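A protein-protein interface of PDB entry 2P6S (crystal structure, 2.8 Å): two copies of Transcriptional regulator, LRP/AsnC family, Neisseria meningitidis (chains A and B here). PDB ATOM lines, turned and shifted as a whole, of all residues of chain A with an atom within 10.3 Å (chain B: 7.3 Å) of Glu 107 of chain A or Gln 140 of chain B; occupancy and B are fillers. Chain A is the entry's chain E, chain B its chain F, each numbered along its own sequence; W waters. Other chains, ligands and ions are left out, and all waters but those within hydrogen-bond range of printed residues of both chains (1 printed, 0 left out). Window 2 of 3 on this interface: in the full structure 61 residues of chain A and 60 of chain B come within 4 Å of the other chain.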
ATOM      1  N   ARG A  75       7.276  17.035 -25.724  1.00  0.00           N
ATOM      2  CA  ARG A  75       8.527  16.657 -25.079  1.00  0.00           C
ATOM      3  C   ARG A  75       9.648  16.845 -26.084  1.00  0.00           C
ATOM      4  O   ARG A  75       9.724  16.118 -27.077  1.00  0.00           O
ATOM      5  CB  ARG A  75       8.486  15.194 -24.626  1.00  0.00           C
ATOM      6  CG  ARG A  75       7.563  14.917 -23.439  1.00  0.00           C
ATOM      7  CD  ARG A  75       6.894  13.535 -23.531  1.00  0.00           C
ATOM      8  NE  ARG A  75       7.844  12.427 -23.706  1.00  0.00           N
ATOM      9  CZ  ARG A  75       8.327  11.648 -22.732  1.00  0.00           C
ATOM     10  NH1 ARG A  75       7.991  11.826 -21.456  1.00  0.00           N
ATOM     11  NH2 ARG A  75       9.180  10.675 -23.038  1.00  0.00           N
ATOM     12  N   VAL A  76      10.511  17.827 -25.825  1.00  0.00           N
ATOM     13  CA  VAL A  76      11.620  18.157 -26.717  1.00  0.00           C
ATOM     14  C   VAL A  76      12.932  17.810 -26.035  1.00  0.00           C
ATOM     15  O   VAL A  76      13.007  17.758 -24.808  1.00  0.00           O
ATOM     16  CB  VAL A  76      11.617  19.665 -27.094  1.00  0.00           C
ATOM     17  CG1 VAL A  76      12.586  19.935 -28.232  1.00  0.00           C
ATOM     18  CG2 VAL A  76      10.223  20.121 -27.488  1.00  0.00           C
ATOM     19  N   SER A  77      13.951  17.548 -26.840  1.00  0.00           N
ATOM     20  CA  SER A  77      15.311  17.374 -26.345  1.00  0.00           C
ATOM     21  C   SER A  77      16.258  18.138 -27.262  1.00  0.00           C
ATOM     22  O   SER A  77      16.215  17.983 -28.488  1.00  0.00           O
ATOM     23  CB  SER A  77      15.684  15.896 -26.296  1.00  0.00           C
ATOM     24  OG  SER A  77      15.429  15.276 -27.542  1.00  0.00           O
ATOM     25  N   ILE A  78      17.116  18.955 -26.661  1.00  0.00           N
ATOM     26  CA  ILE A  78      17.893  19.930 -27.409  1.00  0.00           C
ATOM     27  C   ILE A  78      19.323  19.451 -27.598  1.00  0.00           C
ATOM     28  O   ILE A  78      19.880  18.760 -26.749  1.00  0.00           O
ATOM     29  CB  ILE A  78      17.864  21.308 -26.708  1.00  0.00           C
ATOM     30  CG1 ILE A  78      17.308  22.375 -27.652  1.00  0.00           C
ATOM     31  CG2 ILE A  78      19.241  21.689 -26.185  1.00  0.00           C
ATOM     32  CD1 ILE A  78      15.872  22.109 -28.093  1.00  0.00           C
ATOM     33  N   LYS A  80      23.362  19.164 -27.969  1.00  0.00           N
ATOM     34  CA  LYS A  80      24.343  19.383 -26.920  1.00  0.00           C
ATOM     35  C   LYS A  80      25.425  20.353 -27.390  1.00  0.00           C
ATOM     36  O   LYS A  80      26.438  19.949 -27.966  1.00  0.00           O
ATOM     37  CB  LYS A  80      24.967  18.052 -26.489  1.00  0.00           C
ATOM     38  CG  LYS A  80      23.965  17.001 -25.981  1.00  0.00           C
ATOM     39  CD  LYS A  80      23.278  16.233 -27.121  1.00  0.00           C
ATOM     40  CE  LYS A  80      22.700  14.904 -26.658  1.00  0.00           C
ATOM     41  NZ  LYS A  80      21.973  14.207 -27.750  1.00  0.00           N
ATOM     42  N   PHE A 102       9.350  24.221 -20.015  1.00  0.00           N
ATOM     43  CA  PHE A 102       9.964  23.792 -18.776  1.00  0.00           C
ATOM     44  C   PHE A 102      11.133  22.856 -19.025  1.00  0.00           C
ATOM     45  O   PHE A 102      10.984  21.854 -19.719  1.00  0.00           O
ATOM     46  CB  PHE A 102       8.926  23.066 -17.930  1.00  0.00           C
ATOM     47  CG  PHE A 102       7.769  23.930 -17.513  1.00  0.00           C
ATOM     48  CD1 PHE A 102       7.929  24.906 -16.537  1.00  0.00           C
ATOM     49  CD2 PHE A 102       6.513  23.755 -18.075  1.00  0.00           C
ATOM     50  CE1 PHE A 102       6.864  25.695 -16.142  1.00  0.00           C
ATOM     51  CE2 PHE A 102       5.440  24.543 -17.674  1.00  0.00           C
ATOM     52  CZ  PHE A 102       5.619  25.511 -16.708  1.00  0.00           C
ATOM     53  N   ALA A 103      12.292  23.184 -18.457  1.00  0.00           N
ATOM     54  CA  ALA A 103      13.414  22.252 -18.387  1.00  0.00           C
ATOM     55  C   ALA A 103      13.101  21.265 -17.272  1.00  0.00           C
ATOM     56  O   ALA A 103      12.912  21.676 -16.126  1.00  0.00           O
ATOM     57  CB  ALA A 103      14.703  22.985 -18.095  1.00  0.00           C
ATOM     58  N   LEU A 104      13.027  19.979 -17.613  1.00  0.00           N
ATOM     59  CA  LEU A 104      12.564  18.948 -16.681  1.00  0.00           C
ATOM     60  C   LEU A 104      13.610  17.890 -16.375  1.00  0.00           C
ATOM     61  O   LEU A 104      14.564  17.681 -17.134  1.00  0.00           O
ATOM     62  CB  LEU A 104      11.329  18.228 -17.234  1.00  0.00           C
ATOM     63  CG  LEU A 104       9.953  18.852 -17.026  1.00  0.00           C
ATOM     64  CD1 LEU A 104       8.866  17.802 -17.313  1.00  0.00           C
ATOM     65  CD2 LEU A 104       9.806  19.414 -15.618  1.00  0.00           C
ATOM     66  N   THR A 105      13.392  17.211 -15.254  1.00  0.00           N
ATOM     67  CA  THR A 105      14.127  16.003 -14.936  1.00  0.00           C
ATOM     68  C   THR A 105      13.499  14.819 -15.685  1.00  0.00           C
ATOM     69  O   THR A 105      12.385  14.919 -16.218  1.00  0.00           O
ATOM     70  CB  THR A 105      14.140  15.736 -13.422  1.00  0.00           C
ATOM     71  OG1 THR A 105      12.796  15.642 -12.935  1.00  0.00           O
ATOM     72  CG2 THR A 105      14.861  16.857 -12.699  1.00  0.00           C
ATOM     73  N   GLY A 106      14.234  13.710 -15.734  1.00  0.00           N
ATOM     74  CA  GLY A 106      13.777  12.498 -16.401  1.00  0.00           C
ATOM     75  C   GLY A 106      14.200  12.427 -17.854  1.00  0.00           C
ATOM     76  O   GLY A 106      15.057  13.190 -18.306  1.00  0.00           O
ATOM     77  N   GLU A 107      13.595  11.488 -18.574  1.00  0.00           N
ATOM     78  CA  GLU A 107      13.949  11.203 -19.966  1.00  0.00           C
ATOM     79  C   GLU A 107      13.937  12.432 -20.867  1.00  0.00           C
ATOM     80  O   GLU A 107      14.893  12.656 -21.593  1.00  0.00           O
ATOM     81  CB  GLU A 107      13.058  10.099 -20.551  1.00  0.00           C
ATOM     82  CG  GLU A 107      11.553  10.297 -20.367  1.00  0.00           C
ATOM     83  CD  GLU A 107      10.824   8.974 -20.190  1.00  0.00           C
ATOM     84  OE1 GLU A 107      10.542   8.303 -21.208  1.00  0.00           O
ATOM     85  OE2 GLU A 107      10.543   8.601 -19.030  1.00  0.00           O
ATOM     86  N   THR A 108      12.876  13.232 -20.809  1.00  0.00           N
ATOM     87  CA  THR A 108      12.803  14.445 -21.639  1.00  0.00           C
ATOM     88  C   THR A 108      13.504  15.605 -20.957  1.00  0.00           C
ATOM     89  O   THR A 108      13.412  15.776 -19.735  1.00  0.00           O
ATOM     90  CB  THR A 108      11.358  14.887 -21.951  1.00  0.00           C
ATOM     91  OG1 THR A 108      10.915  15.849 -20.980  1.00  0.00           O
ATOM     92  CG2 THR A 108      10.427  13.693 -21.972  1.00  0.00           C
ATOM     93  N   ASP A 109      14.182  16.415 -21.763  1.00  0.00           N
ATOM     94  CA  ASP A 109      14.963  17.527 -21.242  1.00  0.00           C
ATOM     95  C   ASP A 109      14.121  18.786 -21.167  1.00  0.00           C
ATOM     96  O   ASP A 109      14.250  19.547 -20.218  1.00  0.00           O
ATOM     97  CB  ASP A 109      16.218  17.730 -22.089  1.00  0.00           C
ATOM     98  CG  ASP A 109      17.101  16.495 -22.108  1.00  0.00           C
ATOM     99  OD1 ASP A 109      17.399  15.955 -21.011  1.00  0.00           O
ATOM    100  OD2 ASP A 109      17.478  16.051 -23.216  1.00  0.00           O
ATOM    101  N   TYR A 110      13.254  18.988 -22.156  1.00  0.00           N
ATOM    102  CA  TYR A 110      12.326  20.122 -22.164  1.00  0.00           C
ATOM    103  C   TYR A 110      10.885  19.672 -22.393  1.00  0.00           C
ATOM    104  O   TYR A 110      10.639  18.704 -23.115  1.00  0.00           O
ATOM    105  CB  TYR A 110      12.735  21.145 -23.226  1.00  0.00           C
ATOM    106  CG  TYR A 110      13.936  21.969 -22.818  1.00  0.00           C
ATOM    107  CD1 TYR A 110      13.809  22.982 -21.880  1.00  0.00           C
ATOM    108  CD2 TYR A 110      15.197  21.726 -23.356  1.00  0.00           C
ATOM    109  CE1 TYR A 110      14.898  23.736 -21.488  1.00  0.00           C
ATOM    110  CE2 TYR A 110      16.296  22.478 -22.972  1.00  0.00           C
ATOM    111  CZ  TYR A 110      16.138  23.483 -22.035  1.00  0.00           C
ATOM    112  OH  TYR A 110      17.210  24.247 -21.628  1.00  0.00           O
ATOM    113  N   LEU A 111       9.945  20.375 -21.764  1.00  0.00           N
ATOM    114  CA  LEU A 111       8.519  20.105 -21.919  1.00  0.00           C
ATOM    115  C   LEU A 111       7.834  21.394 -22.339  1.00  0.00           C
ATOM    116  O   LEU A 111       7.928  22.390 -21.634  1.00  0.00           O
ATOM    117  CB  LEU A 111       7.915  19.610 -20.601  1.00  0.00           C
ATOM    118  CG  LEU A 111       6.439  19.184 -20.656  1.00  0.00           C
ATOM    119  CD1 LEU A 111       6.310  17.823 -21.288  1.00  0.00           C
ATOM    120  CD2 LEU A 111       5.814  19.177 -19.278  1.00  0.00           C
ATOM    121  N   ASP A 138      15.304  16.235 -31.205  1.00  0.00           N
ATOM    122  CA  ASP A 138      14.151  15.336 -31.262  1.00  0.00           C
ATOM    123  C   ASP A 138      12.926  15.962 -30.586  1.00  0.00           C
ATOM    124  O   ASP A 138      13.056  16.787 -29.676  1.00  0.00           O
ATOM    125  CB  ASP A 138      14.500  13.997 -30.595  1.00  0.00           C
ATOM    126  CG  ASP A 138      13.377  12.972 -30.703  1.00  0.00           C
ATOM    127  OD1 ASP A 138      12.817  12.811 -31.809  1.00  0.00           O
ATOM    128  OD2 ASP A 138      13.056  12.324 -29.681  1.00  0.00           O
ATOM    129  N   GLN A 140       8.773  14.767 -29.226  1.00  0.00           N
ATOM    130  CA  GLN A 140       7.695  13.801 -29.014  1.00  0.00           C
ATOM    131  C   GLN A 140       6.497  14.568 -28.508  1.00  0.00           C
ATOM    132  O   GLN A 140       6.547  15.102 -27.410  1.00  0.00           O
ATOM    133  CB  GLN A 140       8.084  12.768 -27.957  1.00  0.00           C
ATOM    134  CG  GLN A 140       9.209  11.852 -28.370  1.00  0.00           C
ATOM    135  CD  GLN A 140       9.602  10.885 -27.273  1.00  0.00           C
ATOM    136  OE1 GLN A 140       8.872  10.702 -26.296  1.00  0.00           O
ATOM    137  NE2 GLN A 140      10.762  10.250 -27.434  1.00  0.00           N
ATOM    138  N   PHE B  73       5.547  17.786 -12.497  1.00  0.00           N
ATOM    139  CA  PHE B  73       4.716  17.283 -13.583  1.00  0.00           C
ATOM    140  C   PHE B  73       4.707  15.774 -13.449  1.00  0.00           C
ATOM    141  O   PHE B  73       5.730  15.133 -13.696  1.00  0.00           O
ATOM    142  CB  PHE B  73       5.286  17.665 -14.951  1.00  0.00           C
ATOM    143  CG  PHE B  73       4.988  19.075 -15.359  1.00  0.00           C
ATOM    144  CD1 PHE B  73       3.721  19.420 -15.808  1.00  0.00           C
ATOM    145  CD2 PHE B  73       5.972  20.062 -15.296  1.00  0.00           C
ATOM    146  CE1 PHE B  73       3.434  20.727 -16.182  1.00  0.00           C
ATOM    147  CE2 PHE B  73       5.695  21.372 -15.670  1.00  0.00           C
ATOM    148  CZ  PHE B  73       4.426  21.707 -16.112  1.00  0.00           C
ATOM    149  N   ILE B  74       3.548  15.221 -13.071  1.00  0.00           N
ATOM    150  CA  ILE B  74       3.398  13.797 -12.774  1.00  0.00           C
ATOM    151  C   ILE B  74       2.593  13.056 -13.842  1.00  0.00           C
ATOM    152  O   ILE B  74       1.559  13.533 -14.287  1.00  0.00           O
ATOM    153  CB  ILE B  74       2.697  13.592 -11.430  1.00  0.00           C
ATOM    154  CG1 ILE B  74       3.435  14.347 -10.315  1.00  0.00           C
ATOM    155  CG2 ILE B  74       2.599  12.103 -11.110  1.00  0.00           C
ATOM    156  CD1 ILE B  74       2.794  14.196  -8.932  1.00  0.00           C
ATOM    157  N   ARG B  75       3.078  11.874 -14.217  1.00  0.00           N
ATOM    158  CA  ARG B  75       2.438  11.015 -15.210  1.00  0.00           C
ATOM    159  C   ARG B  75       1.914   9.752 -14.530  1.00  0.00           C
ATOM    160  O   ARG B  75       2.690   8.869 -14.184  1.00  0.00           O
ATOM    161  CB  ARG B  75       3.458  10.629 -16.278  1.00  0.00           C
ATOM    162  CG  ARG B  75       3.968  11.793 -17.116  1.00  0.00           C
ATOM    163  CD  ARG B  75       5.450  11.656 -17.433  1.00  0.00           C
ATOM    164  NE  ARG B  75       5.747  10.441 -18.183  1.00  0.00           N
ATOM    165  CZ  ARG B  75       6.970  10.053 -18.538  1.00  0.00           C
ATOM    166  NH1 ARG B  75       8.039  10.778 -18.213  1.00  0.00           N
ATOM    167  NH2 ARG B  75       7.125   8.926 -19.226  1.00  0.00           N
ATOM    168  N   VAL B  76       0.599   9.664 -14.346  1.00  0.00           N
ATOM    169  CA  VAL B  76      -0.009   8.523 -13.641  1.00  0.00           C
ATOM    170  C   VAL B  76      -0.871   7.711 -14.595  1.00  0.00           C
ATOM    171  O   VAL B  76      -1.455   8.253 -15.527  1.00  0.00           O
ATOM    172  CB  VAL B  76      -0.875   8.948 -12.394  1.00  0.00           C
ATOM    173  CG1 VAL B  76      -0.667  10.417 -12.041  1.00  0.00           C
ATOM    174  CG2 VAL B  76      -2.357   8.667 -12.613  1.00  0.00           C
ATOM    175  N   SER B  77      -0.938   6.409 -14.357  1.00  0.00           N
ATOM    176  CA  SER B  77      -1.830   5.532 -15.100  1.00  0.00           C
ATOM    177  C   SER B  77      -2.837   4.949 -14.127  1.00  0.00           C
ATOM    178  O   SER B  77      -2.578   4.882 -12.927  1.00  0.00           O
ATOM    179  CB  SER B  77      -1.043   4.425 -15.786  1.00  0.00           C
ATOM    180  OG  SER B  77      -0.291   3.693 -14.840  1.00  0.00           O
ATOM    181  N   GLU B 107       2.111   7.228 -24.087  1.00  0.00           N
ATOM    182  CA  GLU B 107       2.386   6.235 -23.057  1.00  0.00           C
ATOM    183  C   GLU B 107       1.524   6.496 -21.837  1.00  0.00           C
ATOM    184  O   GLU B 107       0.831   5.597 -21.365  1.00  0.00           O
ATOM    185  CB  GLU B 107       3.865   6.248 -22.655  1.00  0.00           C
ATOM    186  CG  GLU B 107       4.843   5.888 -23.777  1.00  0.00           C
ATOM    187  CD  GLU B 107       6.222   5.490 -23.258  1.00  0.00           C
ATOM    188  OE1 GLU B 107       6.311   4.506 -22.491  1.00  0.00           O
ATOM    189  OE2 GLU B 107       7.218   6.153 -23.623  1.00  0.00           O
ATOM    190  N   THR B 108       1.545   7.735 -21.353  1.00  0.00           N
ATOM    191  CA  THR B 108       0.835   8.090 -20.120  1.00  0.00           C
ATOM    192  C   THR B 108      -0.652   8.264 -20.392  1.00  0.00           C
ATOM    193  O   THR B 108      -1.045   8.847 -21.405  1.00  0.00           O
ATOM    194  CB  THR B 108       1.346   9.415 -19.470  1.00  0.00           C
ATOM    195  OG1 THR B 108       0.433  10.489 -19.756  1.00  0.00           O
ATOM    196  CG2 THR B 108       2.766   9.779 -19.944  1.00  0.00           C
ATOM    197  N   TYR B 110      -2.632   9.852 -17.962  1.00  0.00           N
ATOM    198  CA  TYR B 110      -2.864  11.180 -17.410  1.00  0.00           C
ATOM    199  C   TYR B 110      -1.570  11.954 -17.139  1.00  0.00           C
ATOM    200  O   TYR B 110      -0.475  11.374 -17.095  1.00  0.00           O
ATOM    201  CB  TYR B 110      -3.698  11.057 -16.145  1.00  0.00           C
ATOM    202  CG  TYR B 110      -5.106  10.619 -16.440  1.00  0.00           C
ATOM    203  CD1 TYR B 110      -6.106  11.555 -16.670  1.00  0.00           C
ATOM    204  CD2 TYR B 110      -5.437   9.267 -16.516  1.00  0.00           C
ATOM    205  CE1 TYR B 110      -7.405  11.166 -16.954  1.00  0.00           C
ATOM    206  CE2 TYR B 110      -6.739   8.862 -16.799  1.00  0.00           C
ATOM    207  CZ  TYR B 110      -7.719   9.818 -17.016  1.00  0.00           C
ATOM    208  OH  TYR B 110      -9.014   9.442 -17.300  1.00  0.00           O
ATOM    209  N   LEU B 111      -1.715  13.273 -16.989  1.00  0.00           N
ATOM    210  CA  LEU B 111      -0.598  14.167 -16.669  1.00  0.00           C
ATOM    211  C   LEU B 111      -1.067  15.314 -15.795  1.00  0.00           C
ATOM    212  O   LEU B 111      -1.874  16.134 -16.238  1.00  0.00           O
ATOM    213  CB  LEU B 111       0.029  14.740 -17.944  1.00  0.00           C
ATOM    214  CG  LEU B 111       1.217  15.694 -17.766  1.00  0.00           C
ATOM    215  CD1 LEU B 111       2.358  15.012 -17.055  1.00  0.00           C
ATOM    216  CD2 LEU B 111       1.673  16.206 -19.119  1.00  0.00           C
ATOM    217  N   PHE B 122       6.325  16.684  -1.183  1.00  0.00           N
ATOM    218  CA  PHE B 122       5.990  15.841  -2.318  1.00  0.00           C
ATOM    219  C   PHE B 122       5.866  14.383  -1.909  1.00  0.00           C
ATOM    220  O   PHE B 122       4.892  13.719  -2.241  1.00  0.00           O
ATOM    221  CB  PHE B 122       7.048  15.956  -3.408  1.00  0.00           C
ATOM    222  CG  PHE B 122       6.636  15.332  -4.704  1.00  0.00           C
ATOM    223  CD1 PHE B 122       5.794  16.011  -5.557  1.00  0.00           C
ATOM    224  CD2 PHE B 122       7.084  14.067  -5.068  1.00  0.00           C
ATOM    225  CE1 PHE B 122       5.398  15.453  -6.758  1.00  0.00           C
ATOM    226  CE2 PHE B 122       6.699  13.499  -6.266  1.00  0.00           C
ATOM    227  CZ  PHE B 122       5.851  14.192  -7.115  1.00  0.00           C
ATOM    228  N   LEU B 130      -1.653  10.265  -3.597  1.00  0.00           N
ATOM    229  CA  LEU B 130      -1.712   9.850  -5.001  1.00  0.00           C
ATOM    230  C   LEU B 130      -1.682   8.312  -5.122  1.00  0.00           C
ATOM    231  O   LEU B 130      -2.633   7.695  -5.614  1.00  0.00           O
ATOM    232  CB  LEU B 130      -0.563  10.477  -5.806  1.00  0.00           C
ATOM    233  CG  LEU B 130      -0.647  10.339  -7.337  1.00  0.00           C
ATOM    234  CD1 LEU B 130      -1.731  11.231  -7.916  1.00  0.00           C
ATOM    235  CD2 LEU B 130       0.692  10.657  -7.985  1.00  0.00           C
ATOM    236  N   LEU B 131      -0.594   7.707  -4.652  1.00  0.00           N
ATOM    237  CA  LEU B 131      -0.373   6.269  -4.807  1.00  0.00           C
ATOM    238  C   LEU B 131      -1.289   5.395  -3.949  1.00  0.00           C
ATOM    239  O   LEU B 131      -1.425   4.200  -4.219  1.00  0.00           O
ATOM    240  CB  LEU B 131       1.091   5.920  -4.511  1.00  0.00           C
ATOM    241  CG  LEU B 131       2.128   6.472  -5.496  1.00  0.00           C
ATOM    242  CD1 LEU B 131       3.514   6.019  -5.076  1.00  0.00           C
ATOM    243  CD2 LEU B 131       1.841   6.044  -6.935  1.00  0.00           C
ATOM    244  N   ASP B 138      -0.043   3.425 -11.150  1.00  0.00           N
ATOM    245  CA  ASP B 138       1.357   3.749 -11.381  1.00  0.00           C
ATOM    246  C   ASP B 138       1.542   5.265 -11.429  1.00  0.00           C
ATOM    247  O   ASP B 138       0.578   5.994 -11.670  1.00  0.00           O
ATOM    248  CB  ASP B 138       1.786   3.120 -12.703  1.00  0.00           C
ATOM    249  CG  ASP B 138       3.256   2.825 -12.763  1.00  0.00           C
ATOM    250  OD1 ASP B 138       4.054   3.781 -12.709  1.00  0.00           O
ATOM    251  OD2 ASP B 138       3.619   1.636 -12.890  1.00  0.00           O
ATOM    252  N   ALA B 139       2.772   5.729 -11.188  1.00  0.00           N
ATOM    253  CA  ALA B 139       3.104   7.162 -11.222  1.00  0.00           C
ATOM    254  C   ALA B 139       4.576   7.410 -11.558  1.00  0.00           C
ATOM    255  O   ALA B 139       5.469   6.775 -11.003  1.00  0.00           O
ATOM    256  CB  ALA B 139       2.768   7.821  -9.889  1.00  0.00           C
ATOM    257  N   GLN B 140       4.813   8.346 -12.469  1.00  0.00           N
ATOM    258  CA  GLN B 140       6.154   8.783 -12.837  1.00  0.00           C
ATOM    259  C   GLN B 140       6.248  10.287 -12.646  1.00  0.00           C
ATOM    260  O   GLN B 140       5.657  11.041 -13.413  1.00  0.00           O
ATOM    261  CB  GLN B 140       6.408   8.497 -14.311  1.00  0.00           C
ATOM    262  CG  GLN B 140       6.676   7.060 -14.655  1.00  0.00           C
ATOM    263  CD  GLN B 140       7.344   6.923 -16.007  1.00  0.00           C
ATOM    264  OE1 GLN B 140       8.320   7.623 -16.306  1.00  0.00           O
ATOM    265  NE2 GLN B 140       6.826   6.020 -16.833  1.00  0.00           N
ATOM    266  N   SER B 141       6.982  10.739 -11.642  1.00  0.00           N
ATOM    267  CA  SER B 141       7.056  12.172 -11.372  1.00  0.00           C
ATOM    268  C   SER B 141       8.346  12.790 -11.912  1.00  0.00           C
ATOM    269  O   SER B 141       9.411  12.173 -11.862  1.00  0.00           O
ATOM    270  CB  SER B 141       6.926  12.432  -9.872  1.00  0.00           C
ATOM    271  OG  SER B 141       5.654  12.022  -9.402  1.00  0.00           O
ATOM    272  N   SER B 142       8.235  14.007 -12.440  1.00  0.00           N
ATOM    273  CA  SER B 142       9.395  14.792 -12.872  1.00  0.00           C
ATOM    274  C   SER B 142       9.211  16.221 -12.413  1.00  0.00           C
ATOM    275  O   SER B 142       8.083  16.690 -12.290  1.00  0.00           O
ATOM    276  CB  SER B 142       9.545  14.766 -14.392  1.00  0.00           C
ATOM    277  OG  SER B 142       8.580  15.601 -15.003  1.00  0.00           O
HETATM  278  O   HOH W   1      10.781  10.006 -16.899  1.00  0.00           O
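The side-chain carboxylate (OE2) of Glu 107 of chain A is in salt-bridge range of the guanidinium group (NH1) of Arg 75 of chain B, at 3.4 Å.
The guanidinium group of Arg 75 of chain A lies close to the guanidinium group of Arg 75 of chain B, at 3.4 Å.
The side-chain carboxylate of Glu 107 of chain A lies within salt-bridge range of the guanidinium group of Arg 75 of chain A (3.3 Å).
The backbone NH (N) of Arg 75 of chain A lies within hydrogen-bond range of the backbone carbonyl oxygen (O) of Gln 140 of chain A (2.7 Å).
N of Leu 111 of chain A is in hydrogen-bond range of O of Phe 102 of chain A (2.7 Å).
The backbone NH (N) of Leu 104 of chain A is in hydrogen-bond range of the backbone carbonyl oxygen (O) of Asp 109 of chain A (2.9 Å).
The backbone NH (N) of Phe 73 of chain B lies within hydrogen-bond range of the backbone carbonyl oxygen (O) of Ser 142 of chain B.
The backbone NH of Gln 140 of chain B lies within hydrogen-bond range of the backbone carbonyl oxygen of Arg 75 of chain B (2.8 Å).
Phe 102 of chain A touches Phe 73 of chain B (CE2 to CZ, 3.4 Å).
Leu 104 of chain A touches Phe 73 of chain B (CD2 to CD2, 3.9 Å).
Ser 142 of chain B touches Leu 104 of chain A (OG to CD1, 3.2 Å).
Thr 105 of chain A touches Ser 142 of chain B (O to CB, 3.4 Å).
Gln 140 of chain B touches Glu 107 of chain A.
Of the printed residues of chain B, Glu 107 of chain A touches Arg 75 (3.4 Å) and Gln 140 (3.6 Å).
Printed residues of chain A within 4 Å of Gln 140 of chain B: Glu 107 (3.6 Å).
No residue of chain A comes within 4 Å of Ile 74 of chain B.
Of chain A, only Arg 75 and Glu 107 come within 4 Å of Arg 75 of chain B.
No residue of chain A comes within 4 Å of Ala 139 of chain B.
No residue of chain A comes within 4 Å of Ser 141 of chain B.
Of the printed residues of chain B, Leu 104 of chain A touches Phe 73 and Ser 142.
Printed residues of chain B within 4 Å of Phe 102 of chain A: Phe 73.
Asp 138 of chain B touches none of the printed residues of chain A.
Phe 122 of chain B touches none of the printed residues of chain A.
The nearest residue of chain B that does not touch Glu 107 of chain A is Glu 107 of chain B (4.6 Å).
The nearest residue of chain A that does not touch Gln 140 of chain B is Arg 75 of chain A (6.7 Å).
The nearest printed residue of chain A that does not touch Ser 142 of chain B is Gly 106 of chain A (5.0 Å).
Printed residues of chain A that touch a printed residue of chain B: Arg 75, Phe 102, Leu 104, Thr 105 and Glu 107.
Hydrophobic or aromatic side chains of chain A within 4 Å of the printed part of chain B: Phe 102 and Leu 104.
Of the 17 printed residues of chain B, 4 touch a printed residue of chain A.
Along chain B the printed residues that touch a printed residue of chain A span positions 73 to 142.
Among the printed residues, Asp or Glu carboxylates within 4 Å of a Lys or Arg side-chain nitrogen of the other chain: Glu 107 of chain A with Arg 75 of chain B (3.4 Å).
Arg 75 of chain A touches its own counterpart, Arg 75 of chain B.
Glu 107 of chain A touches Arg 75 of chain B, but with the chains exchanged Arg 75 of chain A does not touch Glu 107 of chain B (5.0 Å).
Glu 107 of chain A touches Gln 140 of chain B, but with the chains exchanged Gln 140 of chain A does not touch Glu 107 of chain B (5.5 Å).
Water W1 lies within hydrogen-bond range of the side-chain carboxylate (OE2) of Glu 107 of chain A, the guanidinium group (NH1) of Arg 75 of chain B and the side-chain amide oxygen (OE1) of Gln 140 of chain B.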
